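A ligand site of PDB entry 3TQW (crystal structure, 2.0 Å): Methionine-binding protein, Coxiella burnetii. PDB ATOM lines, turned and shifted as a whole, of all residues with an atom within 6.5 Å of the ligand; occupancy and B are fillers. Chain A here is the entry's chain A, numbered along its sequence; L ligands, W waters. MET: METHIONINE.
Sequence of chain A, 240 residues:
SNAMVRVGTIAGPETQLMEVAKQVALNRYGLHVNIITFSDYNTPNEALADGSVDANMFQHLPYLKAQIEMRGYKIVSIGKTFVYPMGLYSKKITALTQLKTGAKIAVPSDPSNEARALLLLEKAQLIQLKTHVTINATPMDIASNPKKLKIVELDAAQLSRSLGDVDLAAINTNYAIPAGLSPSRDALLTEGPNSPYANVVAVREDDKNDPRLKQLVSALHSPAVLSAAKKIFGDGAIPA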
ATOM      1  N   GLU A  14     -10.033  11.519  28.584  1.00  0.00           N
ATOM      2  CA  GLU A  14      -9.385  11.616  27.273  1.00  0.00           C
ATOM      3  C   GLU A  14      -9.048  10.243  26.684  1.00  0.00           C
ATOM      4  O   GLU A  14      -8.980  10.077  25.465  1.00  0.00           O
ATOM      5  CB  GLU A  14      -8.142  12.501  27.338  1.00  0.00           C
ATOM      6  CG  GLU A  14      -8.477  13.954  27.693  1.00  0.00           C
ATOM      7  CD  GLU A  14      -7.251  14.817  27.891  1.00  0.00           C
ATOM      8  OE1 GLU A  14      -6.139  14.356  27.570  1.00  0.00           O
ATOM      9  OE2 GLU A  14      -7.415  15.960  28.357  1.00  0.00           O
ATOM     10  N   TYR A  41       1.438  13.607  33.491  1.00  0.00           N
ATOM     11  CA  TYR A  41       1.709  14.459  32.330  1.00  0.00           C
ATOM     12  C   TYR A  41       3.165  14.322  31.861  1.00  0.00           C
ATOM     13  O   TYR A  41       3.449  14.444  30.661  1.00  0.00           O
ATOM     14  CB  TYR A  41       1.496  15.926  32.698  1.00  0.00           C
ATOM     15  CG  TYR A  41       0.064  16.429  32.743  1.00  0.00           C
ATOM     16  CD1 TYR A  41      -0.992  15.709  32.207  1.00  0.00           C
ATOM     17  CD2 TYR A  41      -0.215  17.676  33.300  1.00  0.00           C
ATOM     18  CE1 TYR A  41      -2.303  16.201  32.237  1.00  0.00           C
ATOM     19  CE2 TYR A  41      -1.507  18.178  33.335  1.00  0.00           C
ATOM     20  CZ  TYR A  41      -2.543  17.454  32.809  1.00  0.00           C
ATOM     21  OH  TYR A  41      -3.806  17.983  32.859  1.00  0.00           O
ATOM     22  N   PHE A  58      -2.237  14.196  24.708  1.00  0.00           N
ATOM     23  CA  PHE A  58      -2.485  14.528  26.109  1.00  0.00           C
ATOM     24  C   PHE A  58      -2.144  15.971  26.488  1.00  0.00           C
ATOM     25  O   PHE A  58      -2.489  16.407  27.587  1.00  0.00           O
ATOM     26  CB  PHE A  58      -1.698  13.585  27.015  1.00  0.00           C
ATOM     27  CG  PHE A  58      -0.260  13.993  27.202  1.00  0.00           C
ATOM     28  CD1 PHE A  58       0.681  13.712  26.227  1.00  0.00           C
ATOM     29  CD2 PHE A  58       0.145  14.656  28.357  1.00  0.00           C
ATOM     30  CE1 PHE A  58       2.004  14.088  26.387  1.00  0.00           C
ATOM     31  CE2 PHE A  58       1.468  15.032  28.516  1.00  0.00           C
ATOM     32  CZ  PHE A  58       2.396  14.750  27.536  1.00  0.00           C
ATOM     33  N   GLN A  59      -1.458  16.688  25.602  1.00  0.00           N
ATOM     34  CA  GLN A  59      -0.858  17.965  25.976  1.00  0.00           C
ATOM     35  C   GLN A  59      -1.168  19.098  25.013  1.00  0.00           C
ATOM     36  O   GLN A  59      -1.550  18.863  23.861  1.00  0.00           O
ATOM     37  CB  GLN A  59       0.668  17.807  26.054  1.00  0.00           C
ATOM     38  CG  GLN A  59       1.338  17.889  24.689  1.00  0.00           C
ATOM     39  CD  GLN A  59       2.706  17.255  24.677  1.00  0.00           C
ATOM     40  OE1 GLN A  59       3.587  17.634  25.446  1.00  0.00           O
ATOM     41  NE2 GLN A  59       2.898  16.275  23.798  1.00  0.00           N
ATOM     42  N   HIS A  60      -0.987  20.329  25.484  1.00  0.00           N
ATOM     43  CA  HIS A  60      -0.997  21.491  24.603  1.00  0.00           C
ATOM     44  C   HIS A  60       0.423  21.892  24.193  1.00  0.00           C
ATOM     45  O   HIS A  60       1.414  21.381  24.718  1.00  0.00           O
ATOM     46  CB  HIS A  60      -1.750  22.676  25.228  1.00  0.00           C
ATOM     47  CG  HIS A  60      -1.395  22.954  26.658  1.00  0.00           C
ATOM     48  ND1 HIS A  60      -0.128  23.322  27.053  1.00  0.00           N
ATOM     49  CD2 HIS A  60      -2.149  22.935  27.782  1.00  0.00           C
ATOM     50  CE1 HIS A  60      -0.110  23.514  28.357  1.00  0.00           C
ATOM     51  NE2 HIS A  60      -1.327  23.290  28.835  1.00  0.00           N
ATOM     52  N   TYR A  63       2.969  23.216  26.880  1.00  0.00           N
ATOM     53  CA  TYR A  63       3.517  22.116  27.663  1.00  0.00           C
ATOM     54  C   TYR A  63       4.604  21.382  26.872  1.00  0.00           C
ATOM     55  O   TYR A  63       5.663  21.062  27.417  1.00  0.00           O
ATOM     56  CB  TYR A  63       2.418  21.139  28.095  1.00  0.00           C
ATOM     57  CG  TYR A  63       2.917  20.118  29.083  1.00  0.00           C
ATOM     58  CD1 TYR A  63       3.558  18.963  28.648  1.00  0.00           C
ATOM     59  CD2 TYR A  63       2.767  20.318  30.449  1.00  0.00           C
ATOM     60  CE1 TYR A  63       4.027  18.012  29.571  1.00  0.00           C
ATOM     61  CE2 TYR A  63       3.226  19.375  31.377  1.00  0.00           C
ATOM     62  CZ  TYR A  63       3.863  18.237  30.925  1.00  0.00           C
ATOM     63  OH  TYR A  63       4.330  17.302  31.831  1.00  0.00           O
ATOM     64  N   LEU A  64       4.346  21.115  25.602  1.00  0.00           N
ATOM     65  CA  LEU A  64       5.314  20.421  24.752  1.00  0.00           C
ATOM     66  C   LEU A  64       6.612  21.220  24.640  1.00  0.00           C
ATOM     67  O   LEU A  64       7.699  20.667  24.802  1.00  0.00           O
ATOM     68  CB  LEU A  64       4.716  20.189  23.366  1.00  0.00           C
ATOM     69  CG  LEU A  64       5.655  19.560  22.329  1.00  0.00           C
ATOM     70  CD1 LEU A  64       6.255  18.262  22.876  1.00  0.00           C
ATOM     71  CD2 LEU A  64       4.904  19.307  21.009  1.00  0.00           C
ATOM     72  N   PHE A  82      -8.685  19.069  20.624  1.00  0.00           N
ATOM     73  CA  PHE A  82      -9.674  19.914  21.257  1.00  0.00           C
ATOM     74  C   PHE A  82      -8.970  20.864  22.210  1.00  0.00           C
ATOM     75  O   PHE A  82      -7.887  20.566  22.703  1.00  0.00           O
ATOM     76  CB  PHE A  82     -10.688  19.088  22.062  1.00  0.00           C
ATOM     77  CG  PHE A  82     -11.465  18.099  21.235  1.00  0.00           C
ATOM     78  CD1 PHE A  82     -12.730  18.418  20.774  1.00  0.00           C
ATOM     79  CD2 PHE A  82     -10.936  16.859  20.923  1.00  0.00           C
ATOM     80  CE1 PHE A  82     -13.451  17.522  20.011  1.00  0.00           C
ATOM     81  CE2 PHE A  82     -11.647  15.955  20.156  1.00  0.00           C
ATOM     82  CZ  PHE A  82     -12.909  16.283  19.704  1.00  0.00           C
ATOM     83  N   VAL A  83      -9.588  22.013  22.466  1.00  0.00           N
ATOM     84  CA  VAL A  83      -9.167  22.849  23.580  1.00  0.00           C
ATOM     85  C   VAL A  83     -10.127  22.594  24.740  1.00  0.00           C
ATOM     86  O   VAL A  83     -11.331  22.435  24.535  1.00  0.00           O
ATOM     87  CB  VAL A  83      -9.137  24.348  23.213  1.00  0.00           C
ATOM     88  CG1 VAL A  83     -10.498  24.803  22.719  1.00  0.00           C
ATOM     89  CG2 VAL A  83      -8.689  25.180  24.416  1.00  0.00           C
ATOM     90  N   TYR A  84      -9.592  22.525  25.948  1.00  0.00           N
ATOM     91  CA  TYR A  84     -10.387  22.222  27.133  1.00  0.00           C
ATOM     92  C   TYR A  84     -10.278  23.383  28.118  1.00  0.00           C
ATOM     93  O   TYR A  84      -9.424  23.369  29.007  1.00  0.00           O
ATOM     94  CB  TYR A  84      -9.878  20.939  27.817  1.00  0.00           C
ATOM     95  CG  TYR A  84      -9.883  19.706  26.939  1.00  0.00           C
ATOM     96  CD1 TYR A  84     -11.053  18.965  26.753  1.00  0.00           C
ATOM     97  CD2 TYR A  84      -8.722  19.265  26.321  1.00  0.00           C
ATOM     98  CE1 TYR A  84     -11.056  17.817  25.963  1.00  0.00           C
ATOM     99  CE2 TYR A  84      -8.715  18.122  25.523  1.00  0.00           C
ATOM    100  CZ  TYR A  84      -9.885  17.407  25.351  1.00  0.00           C
ATOM    101  OH  TYR A  84      -9.899  16.267  24.567  1.00  0.00           O
ATOM    102  N   PRO A  85     -11.133  24.410  27.954  1.00  0.00           N
ATOM    103  CA  PRO A  85     -11.019  25.620  28.772  1.00  0.00           C
ATOM    104  C   PRO A  85     -10.936  25.311  30.251  1.00  0.00           C
ATOM    105  O   PRO A  85     -11.824  24.658  30.803  1.00  0.00           O
ATOM    106  CB  PRO A  85     -12.296  26.386  28.439  1.00  0.00           C
ATOM    107  CG  PRO A  85     -12.587  25.999  27.032  1.00  0.00           C
ATOM    108  CD  PRO A  85     -12.209  24.529  26.956  1.00  0.00           C
ATOM    109  N   MET A  86      -9.874  25.782  30.891  1.00  0.00           N
ATOM    110  CA  MET A  86      -9.600  25.500  32.297  1.00  0.00           C
ATOM    111  C   MET A  86     -10.526  26.270  33.233  1.00  0.00           C
ATOM    112  O   MET A  86     -10.774  27.467  33.037  1.00  0.00           O
ATOM    113  CB  MET A  86      -8.140  25.814  32.619  1.00  0.00           C
ATOM    114  CG  MET A  86      -7.790  25.752  34.096  1.00  0.00           C
ATOM    115  SD  MET A  86      -5.920  26.204  34.414  1.00  0.00           S
ATOM    116  CE  MET A  86      -5.111  24.502  33.932  1.00  0.00           C
ATOM    117  N   ASP A 110       3.674  22.560  37.274  1.00  0.00           N
ATOM    118  CA  ASP A 110       4.486  22.510  36.060  1.00  0.00           C
ATOM    119  C   ASP A 110       4.432  23.880  35.371  1.00  0.00           C
ATOM    120  O   ASP A 110       3.394  24.536  35.389  1.00  0.00           O
ATOM    121  CB  ASP A 110       3.983  21.416  35.129  1.00  0.00           C
ATOM    122  CG  ASP A 110       2.604  21.706  34.573  1.00  0.00           C
ATOM    123  OD1 ASP A 110       1.615  21.443  35.288  1.00  0.00           O
ATOM    124  OD2 ASP A 110       2.523  22.199  33.434  1.00  0.00           O
ATOM    125  N   SER A 112       4.146  25.469  32.374  1.00  0.00           N
ATOM    126  CA  SER A 112       3.168  26.001  31.425  1.00  0.00           C
ATOM    127  C   SER A 112       1.764  26.087  31.997  1.00  0.00           C
ATOM    128  O   SER A 112       1.061  27.066  31.786  1.00  0.00           O
ATOM    129  CB  SER A 112       3.178  25.206  30.120  1.00  0.00           C
ATOM    130  OG  SER A 112       2.680  23.883  30.303  1.00  0.00           O
ATOM    131  N   ASN A 113       1.338  25.056  32.720  1.00  0.00           N
ATOM    132  CA  ASN A 113       0.003  25.107  33.319  1.00  0.00           C
ATOM    133  C   ASN A 113      -0.077  26.020  34.529  1.00  0.00           C
ATOM    134  O   ASN A 113      -1.151  26.512  34.879  1.00  0.00           O
ATOM    135  CB  ASN A 113      -0.524  23.706  33.622  1.00  0.00           C
ATOM    136  CG  ASN A 113      -0.872  22.938  32.352  1.00  0.00           C
ATOM    137  OD1 ASN A 113      -1.856  23.244  31.675  1.00  0.00           O
ATOM    138  ND2 ASN A 113      -0.052  21.952  32.012  1.00  0.00           N
ATOM    139  N   ARG A 116      -0.481  29.312  32.966  1.00  0.00           N
ATOM    140  CA  ARG A 116      -1.853  29.304  32.473  1.00  0.00           C
ATOM    141  C   ARG A 116      -2.850  29.650  33.576  1.00  0.00           C
ATOM    142  O   ARG A 116      -3.758  30.435  33.367  1.00  0.00           O
ATOM    143  CB  ARG A 116      -2.194  27.928  31.887  1.00  0.00           C
ATOM    144  CG  ARG A 116      -3.651  27.749  31.473  1.00  0.00           C
ATOM    145  CD  ARG A 116      -3.883  26.327  30.978  1.00  0.00           C
ATOM    146  NE  ARG A 116      -5.161  26.162  30.287  1.00  0.00           N
ATOM    147  CZ  ARG A 116      -5.559  25.014  29.759  1.00  0.00           C
ATOM    148  NH1 ARG A 116      -4.784  23.943  29.848  1.00  0.00           N
ATOM    149  NH2 ARG A 116      -6.736  24.928  29.134  1.00  0.00           N
ATOM    150  N   ILE A 171      -7.942  23.884  37.904  1.00  0.00           N
ATOM    151  CA  ILE A 171      -7.784  22.455  37.648  1.00  0.00           C
ATOM    152  C   ILE A 171      -7.947  22.123  36.167  1.00  0.00           C
ATOM    153  O   ILE A 171      -8.899  22.557  35.524  1.00  0.00           O
ATOM    154  CB  ILE A 171      -8.813  21.640  38.466  1.00  0.00           C
ATOM    155  CG1 ILE A 171      -8.752  22.032  39.956  1.00  0.00           C
ATOM    156  CG2 ILE A 171      -8.597  20.132  38.266  1.00  0.00           C
ATOM    157  CD1 ILE A 171      -9.737  21.280  40.840  1.00  0.00           C
ATOM    158  N   ASN A 172      -7.019  21.336  35.615  1.00  0.00           N
ATOM    159  CA  ASN A 172      -7.165  20.891  34.228  1.00  0.00           C
ATOM    160  C   ASN A 172      -8.414  20.028  34.110  1.00  0.00           C
ATOM    161  O   ASN A 172      -8.685  19.199  34.963  1.00  0.00           O
ATOM    162  CB  ASN A 172      -5.949  20.077  33.769  1.00  0.00           C
ATOM    163  CG  ASN A 172      -4.660  20.885  33.796  1.00  0.00           C
ATOM    164  OD1 ASN A 172      -4.243  21.445  32.787  1.00  0.00           O
ATOM    165  ND2 ASN A 172      -4.019  20.914  34.954  1.00  0.00           N
ATOM    166  N   THR A 173      -9.149  20.218  33.032  1.00  0.00           N
ATOM    167  CA  THR A 173     -10.395  19.491  32.821  1.00  0.00           C
ATOM    168  C   THR A 173     -10.255  17.961  32.910  1.00  0.00           C
ATOM    169  O   THR A 173     -11.126  17.293  33.461  1.00  0.00           O
ATOM    170  CB  THR A 173     -11.057  19.924  31.506  1.00  0.00           C
ATOM    171  OG1 THR A 173     -11.449  21.300  31.613  1.00  0.00           O
ATOM    172  CG2 THR A 173     -12.275  19.050  31.191  1.00  0.00           C
ATOM    173  N   ASN A 174      -9.167  17.404  32.382  1.00  0.00           N
ATOM    174  CA  ASN A 174      -9.011  15.942  32.425  1.00  0.00           C
ATOM    175  C   ASN A 174      -8.965  15.431  33.867  1.00  0.00           C
ATOM    176  O   ASN A 174      -9.290  14.270  34.120  1.00  0.00           O
ATOM    177  CB  ASN A 174      -7.803  15.462  31.614  1.00  0.00           C
ATOM    178  CG  ASN A 174      -6.477  15.814  32.261  1.00  0.00           C
ATOM    179  OD1 ASN A 174      -6.063  16.973  32.256  1.00  0.00           O
ATOM    180  ND2 ASN A 174      -5.805  14.822  32.820  1.00  0.00           N
ATOM    181  N   TYR A 197      -4.097  26.906  24.240  1.00  0.00           N
ATOM    182  CA  TYR A 197      -4.035  25.608  24.923  1.00  0.00           C
ATOM    183  C   TYR A 197      -4.796  24.463  24.269  1.00  0.00           C
ATOM    184  O   TYR A 197      -5.196  23.518  24.956  1.00  0.00           O
ATOM    185  CB  TYR A 197      -4.431  25.759  26.393  1.00  0.00           C
ATOM    186  CG  TYR A 197      -3.568  26.761  27.106  1.00  0.00           C
ATOM    187  CD1 TYR A 197      -4.080  27.978  27.543  1.00  0.00           C
ATOM    188  CD2 TYR A 197      -2.210  26.514  27.318  1.00  0.00           C
ATOM    189  CE1 TYR A 197      -3.279  28.907  28.184  1.00  0.00           C
ATOM    190  CE2 TYR A 197      -1.406  27.427  27.954  1.00  0.00           C
ATOM    191  CZ  TYR A 197      -1.937  28.621  28.389  1.00  0.00           C
ATOM    192  OH  TYR A 197      -1.126  29.542  29.026  1.00  0.00           O
ATOM    193  N   ALA A 198      -4.994  24.516  22.958  1.00  0.00           N
ATOM    194  CA  ALA A 198      -5.556  23.377  22.237  1.00  0.00           C
ATOM    195  C   ALA A 198      -4.614  22.196  22.424  1.00  0.00           C
ATOM    196  O   ALA A 198      -3.396  22.348  22.391  1.00  0.00           O
ATOM    197  CB  ALA A 198      -5.716  23.698  20.757  1.00  0.00           C
ATOM    198  N   ASN A 199      -5.168  21.008  22.647  1.00  0.00           N
ATOM    199  CA  ASN A 199      -4.330  19.817  22.750  1.00  0.00           C
ATOM    200  C   ASN A 199      -3.934  19.318  21.376  1.00  0.00           C
ATOM    201  O   ASN A 199      -4.563  19.662  20.366  1.00  0.00           O
ATOM    202  CB  ASN A 199      -5.021  18.728  23.569  1.00  0.00           C
ATOM    203  CG  ASN A 199      -5.045  19.061  25.062  1.00  0.00           C
ATOM    204  OD1 ASN A 199      -5.027  20.225  25.463  1.00  0.00           O
ATOM    205  ND2 ASN A 199      -5.084  18.023  25.890  1.00  0.00           N
HETATM  206  N   MET L   1      -5.540  18.043  28.775  1.00  0.00           N
HETATM  207  CA  MET L   1      -4.806  19.058  29.544  1.00  0.00           C
HETATM  208  C   MET L   1      -5.448  20.420  29.330  1.00  0.00           C
HETATM  209  O   MET L   1      -5.882  20.724  28.220  1.00  0.00           O
HETATM  210  CB  MET L   1      -3.335  19.077  29.104  1.00  0.00           C
HETATM  211  CG  MET L   1      -2.422  20.047  29.858  1.00  0.00           C
HETATM  212  SD  MET L   1      -0.714  19.995  29.256  1.00  0.00           S
HETATM  213  CE  MET L   1      -0.277  18.339  29.769  1.00  0.00           C
HETATM  214  OXT MET L   1      -5.551  21.255  30.240  1.00  0.00           O
HETATM  215  O   HOH W   1      -8.026  18.835  30.092  1.00  0.00           O
HETATM  216  O   HOH W   2      -6.985  22.870  26.933  1.00  0.00           O
HETATM  217  O   HOH W   3      -8.220  21.806  30.868  1.00  0.00           O
HETATM  218  O   HOH W   4      -4.354  15.479  29.253  1.00  0.00           O
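An oxygen (OXT) of the ligand is in salt-bridge range of the guanidinium group (NH1) of Arg 116 (2.8 Å).
A sulfur (SD) of the ligand sits close to a ring nitrogen (NE2) of His 60, at 3.4 Å.
N of His 60 lies close to SD of the ligand, 3.8 Å away.
ND2 of Asn 113 lies close to SD of the ligand, at 3.4 Å.
The side-chain amide oxygen of Asn 172 lies close to an oxygen (OXT) of the ligand (2.9 Å).
The side-chain amide nitrogen of Asn 199 lies close to a nitrogen (N) of the ligand (2.9 Å).
The side-chain carboxylate (OE2) of Glu 14 lies within salt-bridge range of a nitrogen (N) of the ligand (2.8 Å).
Tyr 41 touches the ligand.
O of Phe 58 touches CB of the ligand (3.2 Å).
CA of Gln 59 touches CE of the ligand (3.9 Å).
Tyr 63 touches the ligand.
Tyr 84 touches the ligand (CD2 to O, 3.7 Å).
Asn 174 touches the ligand (OD1 to CA, 3.6 Å).
12 residues have an atom within 4 Å of the ligand: Glu 14, Tyr 41, Phe 58, Gln 59, His 60, Tyr 63, Tyr 84, Asn 113, Arg 116, Asn 172, Asn 174 and Asn 199.
Water W2 lies within hydrogen-bond range of O of the ligand (2.7 Å), O of Tyr 197 (2.7 Å), N of Tyr 84 (2.8 Å) and NH2 of Arg 116 (3.0 Å).
Water W3 lies within hydrogen-bond range of O of Tyr 84 (2.7 Å), OXT of the ligand (2.8 Å) and N of Thr 173 (2.8 Å).
Water W4 lies within hydrogen-bond range of the backbone carbonyl oxygen (O) of Phe 58, the side-chain carboxylate (OE1) of Glu 14 and a nitrogen (N) of the ligand.
Water W1 lies within hydrogen-bond range of N of the ligand (2.9 Å), N of Asn 174 (2.9 Å), OE2 of Glu 14 (3.4 Å) and N of Thr 173 (3.4 Å).
OH of Tyr 41 is in hydrogen-bond range of OD1 of Asn 174, at 2.5 Å.
ND2 of Asn 199 sits at hydrogen-bond distance from O of Phe 58 (3.5 Å).
The side-chain hydroxyl of Tyr 63 sits close to the backbone carbonyl oxygen of Tyr 41 (3.2 Å).
The backbone NH of Tyr 63 sits close to the side-chain hydroxyl of Ser 112.
The side-chain amide oxygen (OD1) of Asn 199 sits close to the backbone carbonyl oxygen (O) of Tyr 197, at 3.3 Å.
A ring nitrogen (ND1) of His 60 sits at hydrogen-bond distance from the backbone NH of Tyr 63 (3.1 Å).
The side-chain amide nitrogen (ND2) of Asn 113 sits at hydrogen-bond distance from the side-chain carboxylate (OD2) of Asp 110 (3.0 Å).
NE2 of His 60 is in hydrogen-bond range of OD1 of Asn 113.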
